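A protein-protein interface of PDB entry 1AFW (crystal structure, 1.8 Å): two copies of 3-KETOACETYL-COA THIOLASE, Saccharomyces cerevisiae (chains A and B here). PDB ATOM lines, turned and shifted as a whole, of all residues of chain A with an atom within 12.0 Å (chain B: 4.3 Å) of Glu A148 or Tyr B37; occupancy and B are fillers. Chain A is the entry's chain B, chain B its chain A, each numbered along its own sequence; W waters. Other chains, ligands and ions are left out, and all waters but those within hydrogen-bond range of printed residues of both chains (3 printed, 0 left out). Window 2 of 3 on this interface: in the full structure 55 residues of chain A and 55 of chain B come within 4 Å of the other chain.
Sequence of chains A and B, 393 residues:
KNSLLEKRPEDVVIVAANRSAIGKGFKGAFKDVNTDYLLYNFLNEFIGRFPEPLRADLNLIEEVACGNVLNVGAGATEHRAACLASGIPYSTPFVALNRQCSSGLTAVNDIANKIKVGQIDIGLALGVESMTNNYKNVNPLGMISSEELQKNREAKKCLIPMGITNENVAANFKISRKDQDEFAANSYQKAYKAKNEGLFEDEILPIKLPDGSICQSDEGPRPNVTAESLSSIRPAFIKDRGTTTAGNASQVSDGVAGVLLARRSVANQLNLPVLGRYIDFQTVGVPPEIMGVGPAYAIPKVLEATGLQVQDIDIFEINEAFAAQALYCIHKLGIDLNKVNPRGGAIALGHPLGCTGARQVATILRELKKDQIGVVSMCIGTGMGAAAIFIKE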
ATOM      1  N   LEU A 141       7.417 -25.567 -28.178  1.00  0.00           N
ATOM      2  CA  LEU A 141       6.348 -25.094 -27.324  1.00  0.00           C
ATOM      3  C   LEU A 141       6.859 -24.841 -25.887  1.00  0.00           C
ATOM      4  O   LEU A 141       6.162 -24.230 -25.055  1.00  0.00           O
ATOM      5  CB  LEU A 141       5.182 -26.082 -27.301  1.00  0.00           C
ATOM      6  CG  LEU A 141       4.025 -26.009 -28.307  1.00  0.00           C
ATOM      7  CD1 LEU A 141       4.167 -24.861 -29.305  1.00  0.00           C
ATOM      8  CD2 LEU A 141       3.991 -27.356 -28.995  1.00  0.00           C
ATOM      9  N   MET A 143       9.637 -26.306 -22.515  1.00  0.00           N
ATOM     10  CA  MET A 143      10.005 -27.490 -21.768  1.00  0.00           C
ATOM     11  C   MET A 143       9.332 -27.567 -20.426  1.00  0.00           C
ATOM     12  O   MET A 143       9.663 -28.476 -19.677  1.00  0.00           O
ATOM     13  CB  MET A 143      11.526 -27.593 -21.650  1.00  0.00           C
ATOM     14  CG  MET A 143      12.155 -27.752 -23.034  1.00  0.00           C
ATOM     15  SD  MET A 143      11.550 -29.346 -23.817  1.00  0.00           S
ATOM     16  CE  MET A 143      12.709 -30.502 -22.883  1.00  0.00           C
ATOM     17  N   ILE A 144       8.401 -26.654 -20.116  1.00  0.00           N
ATOM     18  CA  ILE A 144       7.700 -26.709 -18.832  1.00  0.00           C
ATOM     19  C   ILE A 144       6.425 -27.482 -19.113  1.00  0.00           C
ATOM     20  O   ILE A 144       5.607 -27.098 -19.962  1.00  0.00           O
ATOM     21  CB  ILE A 144       7.310 -25.332 -18.252  1.00  0.00           C
ATOM     22  CG1 ILE A 144       8.600 -24.651 -17.772  1.00  0.00           C
ATOM     23  CG2 ILE A 144       6.349 -25.549 -16.995  1.00  0.00           C
ATOM     24  CD1 ILE A 144       8.385 -23.211 -17.389  1.00  0.00           C
ATOM     25  N   SER A 145       6.249 -28.592 -18.409  1.00  0.00           N
ATOM     26  CA  SER A 145       5.062 -29.428 -18.633  1.00  0.00           C
ATOM     27  C   SER A 145       3.717 -29.039 -18.031  1.00  0.00           C
ATOM     28  O   SER A 145       2.685 -29.211 -18.669  1.00  0.00           O
ATOM     29  CB  SER A 145       5.351 -30.815 -18.083  1.00  0.00           C
ATOM     30  OG  SER A 145       5.723 -31.533 -19.177  1.00  0.00           O
ATOM     31  N   SER A 146       3.765 -28.599 -16.779  1.00  0.00           N
ATOM     32  CA  SER A 146       2.586 -28.242 -16.028  1.00  0.00           C
ATOM     33  C   SER A 146       1.966 -26.957 -16.520  1.00  0.00           C
ATOM     34  O   SER A 146       2.624 -25.921 -16.637  1.00  0.00           O
ATOM     35  CB  SER A 146       2.973 -28.147 -14.581  1.00  0.00           C
ATOM     36  OG  SER A 146       2.059 -27.378 -13.844  1.00  0.00           O
ATOM     37  N   GLU A 147       0.674 -27.050 -16.808  1.00  0.00           N
ATOM     38  CA  GLU A 147      -0.101 -25.911 -17.293  1.00  0.00           C
ATOM     39  C   GLU A 147      -0.008 -24.852 -16.214  1.00  0.00           C
ATOM     40  O   GLU A 147       0.174 -23.659 -16.451  1.00  0.00           O
ATOM     41  CB  GLU A 147      -1.553 -26.362 -17.353  1.00  0.00           C
ATOM     42  CG  GLU A 147      -2.212 -26.266 -18.721  1.00  0.00           C
ATOM     43  CD  GLU A 147      -3.642 -25.724 -18.636  1.00  0.00           C
ATOM     44  OE1 GLU A 147      -4.268 -25.854 -17.549  1.00  0.00           O
ATOM     45  OE2 GLU A 147      -4.115 -25.161 -19.658  1.00  0.00           O
ATOM     46  N   GLU A 148      -0.159 -25.328 -14.996  1.00  0.00           N
ATOM     47  CA  GLU A 148      -0.072 -24.510 -13.819  1.00  0.00           C
ATOM     48  C   GLU A 148       1.276 -23.789 -13.824  1.00  0.00           C
ATOM     49  O   GLU A 148       1.269 -22.606 -13.591  1.00  0.00           O
ATOM     50  CB  GLU A 148      -0.160 -25.463 -12.644  1.00  0.00           C
ATOM     51  CG  GLU A 148       0.276 -25.002 -11.282  1.00  0.00           C
ATOM     52  CD  GLU A 148      -0.176 -26.046 -10.285  1.00  0.00           C
ATOM     53  OE1 GLU A 148      -1.195 -26.693 -10.625  1.00  0.00           O
ATOM     54  OE2 GLU A 148       0.478 -26.271  -9.233  1.00  0.00           O
ATOM     55  N   LEU A 149       2.422 -24.435 -14.103  1.00  0.00           N
ATOM     56  CA  LEU A 149       3.690 -23.675 -14.108  1.00  0.00           C
ATOM     57  C   LEU A 149       3.763 -22.801 -15.345  1.00  0.00           C
ATOM     58  O   LEU A 149       4.312 -21.690 -15.304  1.00  0.00           O
ATOM     59  CB  LEU A 149       4.952 -24.557 -14.058  1.00  0.00           C
ATOM     60  CG  LEU A 149       5.090 -24.880 -12.571  1.00  0.00           C
ATOM     61  CD1 LEU A 149       6.054 -26.009 -12.476  1.00  0.00           C
ATOM     62  CD2 LEU A 149       5.561 -23.655 -11.787  1.00  0.00           C
ATOM     63  N   GLN A 150       3.202 -23.305 -16.437  1.00  0.00           N
ATOM     64  CA  GLN A 150       3.216 -22.533 -17.668  1.00  0.00           C
ATOM     65  C   GLN A 150       2.465 -21.180 -17.529  1.00  0.00           C
ATOM     66  O   GLN A 150       2.740 -20.206 -18.230  1.00  0.00           O
ATOM     67  CB  GLN A 150       2.520 -23.290 -18.766  1.00  0.00           C
ATOM     68  CG  GLN A 150       3.229 -24.462 -19.338  1.00  0.00           C
ATOM     69  CD  GLN A 150       2.276 -25.259 -20.200  1.00  0.00           C
ATOM     70  OE1 GLN A 150       1.399 -24.717 -20.857  1.00  0.00           O
ATOM     71  NE2 GLN A 150       2.424 -26.556 -20.191  1.00  0.00           N
ATOM     72  N   LYS A 151       1.523 -21.078 -16.614  1.00  0.00           N
ATOM     73  CA  LYS A 151       0.871 -19.793 -16.549  1.00  0.00           C
ATOM     74  C   LYS A 151       1.387 -19.023 -15.401  1.00  0.00           C
ATOM     75  O   LYS A 151       0.947 -17.878 -15.236  1.00  0.00           O
ATOM     76  CB  LYS A 151      -0.629 -19.955 -16.389  1.00  0.00           C
ATOM     77  CG  LYS A 151      -1.241 -20.794 -17.479  1.00  0.00           C
ATOM     78  CD  LYS A 151      -2.756 -20.694 -17.498  1.00  0.00           C
ATOM     79  CE  LYS A 151      -3.422 -22.045 -17.189  1.00  0.00           C
ATOM     80  NZ  LYS A 151      -4.824 -22.016 -16.614  1.00  0.00           N
ATOM     81  N   ASN A 152       2.296 -19.615 -14.625  1.00  0.00           N
ATOM     82  CA  ASN A 152       2.850 -18.939 -13.460  1.00  0.00           C
ATOM     83  C   ASN A 152       3.662 -17.771 -13.952  1.00  0.00           C
ATOM     84  O   ASN A 152       4.394 -17.904 -14.931  1.00  0.00           O
ATOM     85  CB  ASN A 152       3.655 -19.906 -12.581  1.00  0.00           C
ATOM     86  CG  ASN A 152       4.269 -19.244 -11.378  1.00  0.00           C
ATOM     87  OD1 ASN A 152       5.328 -18.623 -11.467  1.00  0.00           O
ATOM     88  ND2 ASN A 152       3.609 -19.360 -10.218  1.00  0.00           N
ATOM     89  N   ARG A 153       3.487 -16.628 -13.292  1.00  0.00           N
ATOM     90  CA  ARG A 153       4.138 -15.351 -13.649  1.00  0.00           C
ATOM     91  C   ARG A 153       5.646 -15.288 -13.621  1.00  0.00           C
ATOM     92  O   ARG A 153       6.295 -14.549 -14.354  1.00  0.00           O
ATOM     93  CB  ARG A 153       3.598 -14.227 -12.771  1.00  0.00           C
ATOM     94  CG  ARG A 153       4.127 -12.819 -13.129  1.00  0.00           C
ATOM     95  CD  ARG A 153       3.456 -11.750 -12.225  1.00  0.00           C
ATOM     96  NE  ARG A 153       3.701 -12.039 -10.812  1.00  0.00           N
ATOM     97  CZ  ARG A 153       4.839 -11.812 -10.148  1.00  0.00           C
ATOM     98  NH1 ARG A 153       5.920 -11.260 -10.734  1.00  0.00           N
ATOM     99  NH2 ARG A 153       4.883 -12.147  -8.857  1.00  0.00           N
ATOM    100  N   GLU A 154       6.199 -16.048 -12.701  1.00  0.00           N
ATOM    101  CA  GLU A 154       7.628 -16.128 -12.560  1.00  0.00           C
ATOM    102  C   GLU A 154       8.065 -17.310 -13.386  1.00  0.00           C
ATOM    103  O   GLU A 154       9.035 -17.238 -14.127  1.00  0.00           O
ATOM    104  CB  GLU A 154       7.988 -16.421 -11.104  1.00  0.00           C
ATOM    105  CG  GLU A 154       7.594 -15.295 -10.219  1.00  0.00           C
ATOM    106  CD  GLU A 154       8.436 -14.058 -10.517  1.00  0.00           C
ATOM    107  OE1 GLU A 154       9.203 -14.066 -11.512  1.00  0.00           O
ATOM    108  OE2 GLU A 154       8.343 -13.068  -9.742  1.00  0.00           O
ATOM    109  N   ALA A 155       7.386 -18.437 -13.288  1.00  0.00           N
ATOM    110  CA  ALA A 155       7.899 -19.555 -14.082  1.00  0.00           C
ATOM    111  C   ALA A 155       7.930 -19.366 -15.557  1.00  0.00           C
ATOM    112  O   ALA A 155       8.824 -19.887 -16.248  1.00  0.00           O
ATOM    113  CB  ALA A 155       7.153 -20.932 -13.755  1.00  0.00           C
ATOM    114  N   LYS A 156       6.931 -18.640 -16.064  1.00  0.00           N
ATOM    115  CA  LYS A 156       6.900 -18.468 -17.534  1.00  0.00           C
ATOM    116  C   LYS A 156       8.052 -17.609 -18.092  1.00  0.00           C
ATOM    117  O   LYS A 156       8.388 -17.637 -19.282  1.00  0.00           O
ATOM    118  CB  LYS A 156       5.503 -17.998 -17.979  1.00  0.00           C
ATOM    119  CG  LYS A 156       5.117 -16.628 -17.461  1.00  0.00           C
ATOM    120  CD  LYS A 156       4.090 -15.924 -18.399  1.00  0.00           C
ATOM    121  CE  LYS A 156       2.755 -16.599 -18.429  1.00  0.00           C
ATOM    122  NZ  LYS A 156       1.659 -15.655 -18.069  1.00  0.00           N
ATOM    123  N   LYS A 157       8.678 -16.852 -17.195  1.00  0.00           N
ATOM    124  CA  LYS A 157       9.783 -16.036 -17.618  1.00  0.00           C
ATOM    125  C   LYS A 157      10.882 -16.928 -18.149  1.00  0.00           C
ATOM    126  O   LYS A 157      11.696 -16.417 -18.918  1.00  0.00           O
ATOM    127  CB  LYS A 157      10.279 -15.159 -16.496  1.00  0.00           C
ATOM    128  CG  LYS A 157       9.198 -14.165 -15.983  1.00  0.00           C
ATOM    129  CD  LYS A 157       9.564 -13.579 -14.624  1.00  0.00           C
ATOM    130  CE  LYS A 157       8.871 -12.229 -14.425  1.00  0.00           C
ATOM    131  NZ  LYS A 157       8.998 -11.621 -13.062  1.00  0.00           N
ATOM    132  N   CYS A 158      10.892 -18.226 -17.796  1.00  0.00           N
ATOM    133  CA  CYS A 158      11.906 -19.208 -18.291  1.00  0.00           C
ATOM    134  C   CYS A 158      11.550 -19.667 -19.693  1.00  0.00           C
ATOM    135  O   CYS A 158      12.259 -20.444 -20.318  1.00  0.00           O
ATOM    136  CB  CYS A 158      12.179 -20.390 -17.329  1.00  0.00           C
ATOM    137  SG  CYS A 158      12.775 -19.745 -15.731  1.00  0.00           S
ATOM    138  N   LEU A 159      10.441 -19.159 -20.210  1.00  0.00           N
ATOM    139  CA  LEU A 159      10.050 -19.525 -21.576  1.00  0.00           C
ATOM    140  C   LEU A 159      10.251 -18.311 -22.519  1.00  0.00           C
ATOM    141  O   LEU A 159       9.975 -18.350 -23.683  1.00  0.00           O
ATOM    142  CB  LEU A 159       8.604 -20.045 -21.679  1.00  0.00           C
ATOM    143  CG  LEU A 159       8.352 -21.228 -20.758  1.00  0.00           C
ATOM    144  CD1 LEU A 159       6.879 -21.684 -20.809  1.00  0.00           C
ATOM    145  CD2 LEU A 159       9.267 -22.320 -21.322  1.00  0.00           C
ATOM    146  N   VAL B  33       1.727 -36.357 -13.649  1.00  0.00           N
ATOM    147  CA  VAL B  33       2.416 -35.092 -13.434  1.00  0.00           C
ATOM    148  C   VAL B  33       3.900 -35.320 -13.797  1.00  0.00           C
ATOM    149  O   VAL B  33       4.344 -36.452 -13.738  1.00  0.00           O
ATOM    150  CB  VAL B  33       2.193 -34.497 -11.982  1.00  0.00           C
ATOM    151  CG1 VAL B  33       0.638 -34.385 -11.727  1.00  0.00           C
ATOM    152  CG2 VAL B  33       2.879 -35.353 -10.847  1.00  0.00           C
ATOM    153  N   ASN B  34       4.638 -34.261 -14.136  1.00  0.00           N
ATOM    154  CA  ASN B  34       6.075 -34.307 -14.481  1.00  0.00           C
ATOM    155  C   ASN B  34       6.959 -33.743 -13.339  1.00  0.00           C
ATOM    156  O   ASN B  34       6.501 -33.271 -12.275  1.00  0.00           O
ATOM    157  CB  ASN B  34       6.377 -33.596 -15.832  1.00  0.00           C
ATOM    158  CG  ASN B  34       7.382 -34.356 -16.697  1.00  0.00           C
ATOM    159  OD1 ASN B  34       8.281 -35.026 -16.193  1.00  0.00           O
ATOM    160  ND2 ASN B  34       7.216 -34.281 -18.002  1.00  0.00           N
ATOM    161  N   THR B  35       8.264 -33.790 -13.605  1.00  0.00           N
ATOM    162  CA  THR B  35       9.226 -33.302 -12.657  1.00  0.00           C
ATOM    163  C   THR B  35       9.019 -31.855 -12.243  1.00  0.00           C
ATOM    164  O   THR B  35       9.257 -31.491 -11.089  1.00  0.00           O
ATOM    165  CB  THR B  35      10.675 -33.565 -13.106  1.00  0.00           C
ATOM    166  OG1 THR B  35      11.008 -32.730 -14.266  1.00  0.00           O
ATOM    167  CG2 THR B  35      10.840 -35.049 -13.501  1.00  0.00           C
ATOM    168  N   ASP B  36       8.580 -31.013 -13.173  1.00  0.00           N
ATOM    169  CA  ASP B  36       8.378 -29.597 -12.836  1.00  0.00           C
ATOM    170  C   ASP B  36       7.285 -29.526 -11.751  1.00  0.00           C
ATOM    171  O   ASP B  36       7.430 -28.805 -10.735  1.00  0.00           O
ATOM    172  CB  ASP B  36       8.048 -28.782 -14.097  1.00  0.00           C
ATOM    173  CG  ASP B  36       6.786 -29.309 -14.844  1.00  0.00           C
ATOM    174  OD1 ASP B  36       6.418 -30.503 -14.842  1.00  0.00           O
ATOM    175  OD2 ASP B  36       6.104 -28.507 -15.491  1.00  0.00           O
ATOM    176  N   TYR B  37       6.189 -30.286 -11.925  1.00  0.00           N
ATOM    177  CA  TYR B  37       5.120 -30.282 -10.900  1.00  0.00           C
ATOM    178  C   TYR B  37       5.577 -30.874  -9.533  1.00  0.00           C
ATOM    179  O   TYR B  37       5.304 -30.287  -8.449  1.00  0.00           O
ATOM    180  CB  TYR B  37       3.949 -31.100 -11.464  1.00  0.00           C
ATOM    181  CG  TYR B  37       2.724 -31.087 -10.560  1.00  0.00           C
ATOM    182  CD1 TYR B  37       2.623 -31.944  -9.439  1.00  0.00           C
ATOM    183  CD2 TYR B  37       1.687 -30.194 -10.825  1.00  0.00           C
ATOM    184  CE1 TYR B  37       1.520 -31.893  -8.623  1.00  0.00           C
ATOM    185  CE2 TYR B  37       0.558 -30.142 -10.030  1.00  0.00           C
ATOM    186  CZ  TYR B  37       0.468 -30.992  -8.948  1.00  0.00           C
ATOM    187  OH  TYR B  37      -0.685 -30.869  -8.182  1.00  0.00           O
ATOM    188  N   LEU B  38       6.354 -31.959  -9.584  1.00  0.00           N
ATOM    189  CA  LEU B  38       6.863 -32.562  -8.375  1.00  0.00           C
ATOM    190  C   LEU B  38       7.746 -31.580  -7.656  1.00  0.00           C
ATOM    191  O   LEU B  38       7.608 -31.300  -6.433  1.00  0.00           O
ATOM    192  CB  LEU B  38       7.650 -33.861  -8.621  1.00  0.00           C
ATOM    193  CG  LEU B  38       6.751 -34.970  -9.158  1.00  0.00           C
ATOM    194  CD1 LEU B  38       7.519 -36.299  -9.585  1.00  0.00           C
ATOM    195  CD2 LEU B  38       5.623 -35.312  -8.098  1.00  0.00           C
ATOM    196  N   LEU B  39       8.680 -31.007  -8.409  1.00  0.00           N
ATOM    197  CA  LEU B  39       9.540 -30.092  -7.718  1.00  0.00           C
ATOM    198  C   LEU B  39       8.847 -28.869  -7.125  1.00  0.00           C
ATOM    199  O   LEU B  39       9.094 -28.454  -5.967  1.00  0.00           O
ATOM    200  CB  LEU B  39      10.675 -29.704  -8.670  1.00  0.00           C
ATOM    201  CG  LEU B  39      11.736 -28.913  -7.921  1.00  0.00           C
ATOM    202  CD1 LEU B  39      12.300 -29.862  -6.824  1.00  0.00           C
ATOM    203  CD2 LEU B  39      12.783 -28.615  -9.014  1.00  0.00           C
ATOM    204  N   TYR B  40       7.957 -28.254  -7.907  1.00  0.00           N
ATOM    205  CA  TYR B  40       7.256 -27.065  -7.358  1.00  0.00           C
ATOM    206  C   TYR B  40       6.451 -27.348  -6.080  1.00  0.00           C
ATOM    207  O   TYR B  40       6.513 -26.612  -5.073  1.00  0.00           O
ATOM    208  CB  TYR B  40       6.267 -26.632  -8.423  1.00  0.00           C
ATOM    209  CG  TYR B  40       5.284 -25.562  -8.055  1.00  0.00           C
ATOM    210  CD1 TYR B  40       5.713 -24.323  -7.519  1.00  0.00           C
ATOM    211  CD2 TYR B  40       3.932 -25.771  -8.292  1.00  0.00           C
ATOM    212  CE1 TYR B  40       4.799 -23.335  -7.220  1.00  0.00           C
ATOM    213  CE2 TYR B  40       3.040 -24.768  -8.020  1.00  0.00           C
ATOM    214  CZ  TYR B  40       3.465 -23.576  -7.504  1.00  0.00           C
ATOM    215  OH  TYR B  40       2.498 -22.625  -7.233  1.00  0.00           O
ATOM    216  N   ASN B  41       5.669 -28.417  -6.167  1.00  0.00           N
ATOM    217  CA  ASN B  41       4.822 -28.821  -5.042  1.00  0.00           C
ATOM    218  C   ASN B  41       5.633 -29.274  -3.845  1.00  0.00           C
ATOM    219  O   ASN B  41       5.306 -28.963  -2.668  1.00  0.00           O
ATOM    220  CB  ASN B  41       3.836 -29.854  -5.534  1.00  0.00           C
ATOM    221  CG  ASN B  41       2.711 -29.197  -6.259  1.00  0.00           C
ATOM    222  OD1 ASN B  41       1.803 -28.685  -5.602  1.00  0.00           O
ATOM    223  ND2 ASN B  41       2.814 -29.082  -7.598  1.00  0.00           N
ATOM    224  N   LYS B 208      -0.179 -32.592  -3.236  1.00  0.00           N
ATOM    225  CA  LYS B 208      -1.539 -32.824  -3.703  1.00  0.00           C
ATOM    226  C   LYS B 208      -1.460 -32.779  -5.173  1.00  0.00           C
ATOM    227  O   LYS B 208      -0.756 -31.910  -5.692  1.00  0.00           O
ATOM    228  CB  LYS B 208      -2.499 -31.744  -3.256  1.00  0.00           C
ATOM    229  CG  LYS B 208      -3.899 -31.991  -3.850  1.00  0.00           C
ATOM    230  CD  LYS B 208      -5.036 -31.195  -3.170  1.00  0.00           C
ATOM    231  CE  LYS B 208      -4.709 -29.721  -2.967  1.00  0.00           C
ATOM    232  NZ  LYS B 208      -3.835 -29.450  -1.778  1.00  0.00           N
ATOM    233  N   LEU B 209      -2.171 -33.722  -5.791  1.00  0.00           N
ATOM    234  CA  LEU B 209      -2.278 -33.909  -7.225  1.00  0.00           C
ATOM    235  C   LEU B 209      -3.264 -32.897  -7.828  1.00  0.00           C
ATOM    236  O   LEU B 209      -4.063 -32.301  -7.107  1.00  0.00           O
ATOM    237  CB  LEU B 209      -2.678 -35.343  -7.519  1.00  0.00           C
ATOM    238  CG  LEU B 209      -1.534 -36.363  -7.355  1.00  0.00           C
ATOM    239  CD1 LEU B 209      -0.383 -36.026  -8.276  1.00  0.00           C
ATOM    240  CD2 LEU B 209      -0.971 -36.244  -5.976  1.00  0.00           C
ATOM    241  N   PRO B 210      -3.178 -32.676  -9.132  1.00  0.00           N
ATOM    242  CA  PRO B 210      -4.040 -31.685  -9.763  1.00  0.00           C
ATOM    243  C   PRO B 210      -5.502 -31.948  -9.479  1.00  0.00           C
ATOM    244  O   PRO B 210      -6.233 -31.034  -9.059  1.00  0.00           O
ATOM    245  CB  PRO B 210      -3.697 -31.815 -11.265  1.00  0.00           C
ATOM    246  CG  PRO B 210      -2.288 -32.529 -11.275  1.00  0.00           C
ATOM    247  CD  PRO B 210      -2.438 -33.487 -10.127  1.00  0.00           C
HETATM  248  O   HOH W   1       3.096 -19.972  -7.521  1.00  0.00           O
HETATM  249  O   HOH W   2       1.053 -21.194  -9.582  1.00  0.00           O
HETATM  250  O   HOH W   3       8.369 -29.942 -17.494  1.00  0.00           O
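Water W3 lies within hydrogen-bond range of N of Ser A145, O of Met A143 and OD1 of Asp B36.
Water W1 bridges the side-chain hydroxyl of Tyr B40 (2.7 Å) and the side-chain amide nitrogen of Asn A152 (2.8 Å).
Water W2 bridges the side-chain hydroxyl (OH) of Tyr B40 and the side-chain amide nitrogen (ND2) of Asn A152.
No position is printed for both chains.
Of the 7 pairs that touch across the chains among the printed residues, none has its exchanged pair printed and touching as well.
Among the printed residues, merely in contact across the chains: Ile A144 with Asp B36, Glu A148 with Tyr B37, Glu A148 with Tyr B40 and Leu A149 with Asp B36.
Of the printed residues of chain B, Glu A148 touches Tyr B37 and Tyr B40.
No residue of chain A comes within 4 Å of Val B33.
Asp B36 touches just these residues of chain A: Ile A144, Ser A145, Ser A146 and Leu A149.
Printed residues of chain A within 4 Å of Tyr B40: Glu A148.
No residue of chain A comes within 4 Å of Lys B208.
Printed residues of chain B within 4 Å of Ser A146: Asp B36.
Of the printed residues of chain B, Leu A149 touches Asp B36.
Printed residues of chain B within 4 Å of Ser A145: Asn B34 and Asp B36.
Printed residues of chain B within 4 Å of Ile A144: Asp B36.
Asn A152 touches none of the printed residues of chain B.
The nearest printed residue of chain B that does not touch Glu A148 is Asn B41 (4.004 Å).
The nearest printed residue of chain B that does not touch Ser A146 is Tyr B37 (4.1 Å).
OG of Ser A145 lies within hydrogen-bond range of ND2 of Asn B34 (3.3 Å).
The side-chain carboxylate (OD2) of Asp B36 lies within hydrogen-bond range of the backbone NH (N) of Ser A145, 2.9 Å away.
OD2 of Asp B36 sits at hydrogen-bond distance from N of Ser A146, at 2.7 Å.
ND2 of Asn B41 lies within hydrogen-bond range of O of Tyr B37, 2.9 Å away.
The side-chain hydroxyl of Tyr B37 sits at hydrogen-bond distance from the backbone carbonyl oxygen of Lys B208, at 2.7 Å.
The backbone carbonyl oxygen (O) of Ile A144 sits at hydrogen-bond distance from the side-chain amide nitrogen (NE2) of Gln A150, 3.2 Å away.
The side-chain amide nitrogen (NE2) of Gln A150 is in hydrogen-bond range of the backbone carbonyl oxygen (O) of Ser A145.
The side-chain hydroxyl (OG) of Ser A146 lies close to the backbone NH (N) of Glu A148.
The backbone NH (N) of Leu A149 sits at hydrogen-bond distance from the side-chain hydroxyl (OG) of Ser A146 (3.0 Å).
Of the 18 printed residues of chain A, 5 touch a printed residue of chain B.
Printed residues of chain A that touch a printed residue of chain B: Ile A144, Ser A145, Ser A146, Glu A148 and Leu A149.
Printed residues of chain B that touch a printed residue of chain A: Asn B34, Asp B36, Tyr B37 and Tyr B40.
Hydrophobic or aromatic side chains of chain B within 4 Å of the printed part of chain A: Tyr B37 and Tyr B40.
Among the printed residues, 7 pairs touch across the chains.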
